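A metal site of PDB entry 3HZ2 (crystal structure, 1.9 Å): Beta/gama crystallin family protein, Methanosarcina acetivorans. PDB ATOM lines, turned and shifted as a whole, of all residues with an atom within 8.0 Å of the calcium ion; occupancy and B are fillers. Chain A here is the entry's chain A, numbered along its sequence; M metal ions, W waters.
The side-chain amide oxygen (OD1) of Asn 76 is bound to the calcium ion (2.4 Å). The calcium ion is bound by OG of Ser 36 (2.5 Å). O of Glu 9 binds the calcium ion (2.5 Å). The calcium ion is bound by the backbone carbonyl oxygen (O) of Lys 34 (2.5 Å). The calcium ion is bound by water W3. Water W1 is bound to the calcium ion (2.7 Å). The calcium ion is bound by water W2, at 2.7 Å.
Water W1 bridges the side-chain carboxylate of Asp 75 (2.5 Å) and the side-chain amide nitrogen of Asn 76 (3.4 Å).
O of Gly 14 sits at hydrogen-bond distance from N of Glu 9. O of Ile 35 lies within hydrogen-bond range of N of Asn 76. OG of Ser 36 lies close to OD1 of Asp 75, 2.5 Å away. The backbone carbonyl oxygen (O) of Ser 36 lies within hydrogen-bond range of the backbone NH (N) of Val 68 (2.8 Å). The side-chain amide oxygen (OD1) of Asn 76 lies close to the side-chain carboxylate (OD1) of Asp 75, 3.5 Å away. N of Ser 36 sits at hydrogen-bond distance from O of Tyr 8, 2.9 Å away.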
ATOM      1  N   TYR A   8     -27.122 -18.633 -16.572  1.00  0.00           N
ATOM      2  CA  TYR A   8     -26.635 -19.989 -16.827  1.00  0.00           C
ATOM      3  C   TYR A   8     -25.343 -20.320 -16.114  1.00  0.00           C
ATOM      4  O   TYR A   8     -24.483 -19.453 -15.919  1.00  0.00           O
ATOM      5  CB  TYR A   8     -26.435 -20.192 -18.327  1.00  0.00           C
ATOM      6  CG  TYR A   8     -27.646 -19.890 -19.166  1.00  0.00           C
ATOM      7  CD1 TYR A   8     -27.994 -18.571 -19.455  1.00  0.00           C
ATOM      8  CD2 TYR A   8     -28.426 -20.913 -19.684  1.00  0.00           C
ATOM      9  CE1 TYR A   8     -29.102 -18.289 -20.246  1.00  0.00           C
ATOM     10  CE2 TYR A   8     -29.531 -20.645 -20.486  1.00  0.00           C
ATOM     11  CZ  TYR A   8     -29.867 -19.330 -20.756  1.00  0.00           C
ATOM     12  OH  TYR A   8     -30.951 -19.051 -21.563  1.00  0.00           O
ATOM     13  N   GLU A   9     -25.207 -21.584 -15.755  1.00  0.00           N
ATOM     14  CA  GLU A   9     -24.034 -22.096 -15.062  1.00  0.00           C
ATOM     15  C   GLU A   9     -22.759 -21.995 -15.902  1.00  0.00           C
ATOM     16  O   GLU A   9     -21.753 -21.538 -15.422  1.00  0.00           O
ATOM     17  CB  GLU A   9     -24.273 -23.550 -14.653  1.00  0.00           C
ATOM     18  CG  GLU A   9     -23.153 -24.164 -13.825  1.00  0.00           C
ATOM     19  CD  GLU A   9     -23.425 -25.608 -13.447  1.00  0.00           C
ATOM     20  OE1 GLU A   9     -22.605 -26.186 -12.710  1.00  0.00           O
ATOM     21  OE2 GLU A   9     -24.446 -26.163 -13.898  1.00  0.00           O
ATOM     22  N   HIS A  10     -22.809 -22.430 -17.159  1.00  0.00           N
ATOM     23  CA  HIS A  10     -21.608 -22.384 -17.991  1.00  0.00           C
ATOM     24  C   HIS A  10     -21.671 -21.300 -19.055  1.00  0.00           C
ATOM     25  O   HIS A  10     -22.743 -20.779 -19.366  1.00  0.00           O
ATOM     26  CB  HIS A  10     -21.377 -23.723 -18.681  1.00  0.00           C
ATOM     27  CG  HIS A  10     -21.457 -24.914 -17.774  1.00  0.00           C
ATOM     28  ND1 HIS A  10     -20.839 -24.964 -16.545  1.00  0.00           N
ATOM     29  CD2 HIS A  10     -22.065 -26.117 -17.935  1.00  0.00           C
ATOM     30  CE1 HIS A  10     -21.057 -26.138 -15.990  1.00  0.00           C
ATOM     31  NE2 HIS A  10     -21.802 -26.857 -16.811  1.00  0.00           N
ATOM     32  N   VAL A  11     -20.517 -20.978 -19.627  1.00  0.00           N
ATOM     33  CA  VAL A  11     -20.473 -19.991 -20.695  1.00  0.00           C
ATOM     34  C   VAL A  11     -21.254 -20.600 -21.858  1.00  0.00           C
ATOM     35  O   VAL A  11     -21.478 -21.813 -21.896  1.00  0.00           O
ATOM     36  CB  VAL A  11     -19.018 -19.699 -21.155  1.00  0.00           C
ATOM     37  CG1 VAL A  11     -18.253 -19.018 -20.030  1.00  0.00           C
ATOM     38  CG2 VAL A  11     -18.338 -20.975 -21.587  1.00  0.00           C
ATOM     39  N   GLY A  14     -24.734 -22.831 -21.021  1.00  0.00           N
ATOM     40  CA  GLY A  14     -24.784 -24.233 -20.662  1.00  0.00           C
ATOM     41  C   GLY A  14     -25.014 -24.476 -19.185  1.00  0.00           C
ATOM     42  O   GLY A  14     -25.043 -23.537 -18.381  1.00  0.00           O
ATOM     43  N   LEU A  31     -27.461 -21.292  -7.978  1.00  0.00           N
ATOM     44  CA  LEU A  31     -26.548 -20.703  -8.950  1.00  0.00           C
ATOM     45  C   LEU A  31     -25.660 -19.634  -8.334  1.00  0.00           C
ATOM     46  O   LEU A  31     -25.060 -18.831  -9.051  1.00  0.00           O
ATOM     47  CB  LEU A  31     -27.337 -20.105 -10.111  1.00  0.00           C
ATOM     48  CG  LEU A  31     -27.903 -21.154 -11.078  1.00  0.00           C
ATOM     49  CD1 LEU A  31     -28.866 -20.498 -12.058  1.00  0.00           C
ATOM     50  CD2 LEU A  31     -26.761 -21.817 -11.825  1.00  0.00           C
ATOM     51  N   ASP A  33     -22.506 -17.967  -7.100  1.00  0.00           N
ATOM     52  CA  ASP A  33     -21.099 -18.146  -7.446  1.00  0.00           C
ATOM     53  C   ASP A  33     -20.873 -19.155  -8.558  1.00  0.00           C
ATOM     54  O   ASP A  33     -19.873 -19.885  -8.534  1.00  0.00           O
ATOM     55  CB  ASP A  33     -20.297 -18.535  -6.211  1.00  0.00           C
ATOM     56  CG  ASP A  33     -20.185 -17.401  -5.228  1.00  0.00           C
ATOM     57  OD1 ASP A  33     -20.240 -16.261  -5.717  1.00  0.00           O
ATOM     58  OD2 ASP A  33     -20.038 -17.638  -4.021  1.00  0.00           O
ATOM     59  N   LYS A  34     -21.776 -19.189  -9.530  1.00  0.00           N
ATOM     60  CA  LYS A  34     -21.668 -20.106 -10.653  1.00  0.00           C
ATOM     61  C   LYS A  34     -22.017 -19.478 -12.010  1.00  0.00           C
ATOM     62  O   LYS A  34     -21.618 -19.994 -13.039  1.00  0.00           O
ATOM     63  CB  LYS A  34     -22.593 -21.311 -10.474  1.00  0.00           C
ATOM     64  CG  LYS A  34     -22.372 -22.148  -9.236  1.00  0.00           C
ATOM     65  CD  LYS A  34     -23.312 -23.343  -9.279  1.00  0.00           C
ATOM     66  CE  LYS A  34     -23.340 -24.111  -7.989  1.00  0.00           C
ATOM     67  NZ  LYS A  34     -24.316 -25.228  -8.082  1.00  0.00           N
ATOM     68  N   ILE A  35     -22.768 -18.390 -12.012  1.00  0.00           N
ATOM     69  CA  ILE A  35     -23.187 -17.782 -13.274  1.00  0.00           C
ATOM     70  C   ILE A  35     -22.056 -17.367 -14.217  1.00  0.00           C
ATOM     71  O   ILE A  35     -21.162 -16.605 -13.846  1.00  0.00           O
ATOM     72  CB  ILE A  35     -24.129 -16.595 -13.019  1.00  0.00           C
ATOM     73  CG1 ILE A  35     -25.387 -17.084 -12.306  1.00  0.00           C
ATOM     74  CG2 ILE A  35     -24.497 -15.917 -14.341  1.00  0.00           C
ATOM     75  CD1 ILE A  35     -26.262 -15.983 -11.740  1.00  0.00           C
ATOM     76  N   SER A  36     -22.124 -17.860 -15.455  1.00  0.00           N
ATOM     77  CA  SER A  36     -21.113 -17.591 -16.480  1.00  0.00           C
ATOM     78  C   SER A  36     -21.638 -17.004 -17.787  1.00  0.00           C
ATOM     79  O   SER A  36     -20.861 -16.517 -18.603  1.00  0.00           O
ATOM     80  CB  SER A  36     -20.334 -18.855 -16.783  1.00  0.00           C
ATOM     81  OG  SER A  36     -19.610 -19.236 -15.648  1.00  0.00           O
ATOM     82  N   SER A  37     -22.945 -17.083 -17.987  1.00  0.00           N
ATOM     83  CA  SER A  37     -23.553 -16.502 -19.182  1.00  0.00           C
ATOM     84  C   SER A  37     -24.940 -16.016 -18.786  1.00  0.00           C
ATOM     85  O   SER A  37     -25.547 -16.538 -17.839  1.00  0.00           O
ATOM     86  CB  SER A  37     -23.614 -17.524 -20.340  1.00  0.00           C
ATOM     87  OG  SER A  37     -24.304 -18.703 -19.980  1.00  0.00           O
ATOM     88  N   VAL A  68     -20.033 -13.832 -19.010  1.00  0.00           N
ATOM     89  CA  VAL A  68     -20.257 -12.691 -18.133  1.00  0.00           C
ATOM     90  C   VAL A  68     -19.092 -11.699 -18.171  1.00  0.00           C
ATOM     91  O   VAL A  68     -19.275 -10.504 -17.978  1.00  0.00           O
ATOM     92  CB  VAL A  68     -20.486 -13.121 -16.659  1.00  0.00           C
ATOM     93  CG1 VAL A  68     -21.838 -13.811 -16.536  1.00  0.00           C
ATOM     94  CG2 VAL A  68     -19.375 -14.047 -16.204  1.00  0.00           C
ATOM     95  N   ASP A  75     -16.055 -14.167 -13.546  1.00  0.00           N
ATOM     96  CA  ASP A  75     -16.748 -15.456 -13.657  1.00  0.00           C
ATOM     97  C   ASP A  75     -17.013 -16.096 -12.291  1.00  0.00           C
ATOM     98  O   ASP A  75     -16.225 -15.947 -11.364  1.00  0.00           O
ATOM     99  CB  ASP A  75     -15.931 -16.402 -14.550  1.00  0.00           C
ATOM    100  CG  ASP A  75     -16.714 -17.631 -14.947  1.00  0.00           C
ATOM    101  OD1 ASP A  75     -17.943 -17.509 -15.155  1.00  0.00           O
ATOM    102  OD2 ASP A  75     -16.109 -18.713 -15.073  1.00  0.00           O
ATOM    103  N   ASN A  76     -18.137 -16.805 -12.185  1.00  0.00           N
ATOM    104  CA  ASN A  76     -18.519 -17.490 -10.950  1.00  0.00           C
ATOM    105  C   ASN A  76     -18.535 -16.579  -9.725  1.00  0.00           C
ATOM    106  O   ASN A  76     -18.130 -16.998  -8.643  1.00  0.00           O
ATOM    107  CB  ASN A  76     -17.566 -18.653 -10.672  1.00  0.00           C
ATOM    108  CG  ASN A  76     -17.563 -19.660 -11.792  1.00  0.00           C
ATOM    109  OD1 ASN A  76     -18.522 -19.729 -12.535  1.00  0.00           O
ATOM    110  ND2 ASN A  76     -16.506 -20.461 -11.886  1.00  0.00           N
ATOM    111  N   SER A  77     -19.007 -15.360  -9.893  1.00  0.00           N
ATOM    112  CA  SER A  77     -19.002 -14.424  -8.768  1.00  0.00           C
ATOM    113  C   SER A  77     -20.348 -13.785  -8.427  1.00  0.00           C
ATOM    114  O   SER A  77     -20.486 -13.199  -7.365  1.00  0.00           O
ATOM    115  CB  SER A  77     -17.987 -13.319  -9.029  1.00  0.00           C
ATOM    116  OG  SER A  77     -18.407 -12.520 -10.126  1.00  0.00           O
HETATM  117 CA    CA M   1     -19.650 -21.169 -14.092  1.00  0.00          CA
HETATM  118  O   HOH W   1     -17.201 -20.973 -15.164  1.00  0.00           O
HETATM  119  O   HOH W   2     -19.088 -23.479 -15.332  1.00  0.00           O
HETATM  120  O   HOH W   3     -19.628 -22.844 -12.144  1.00  0.00           O
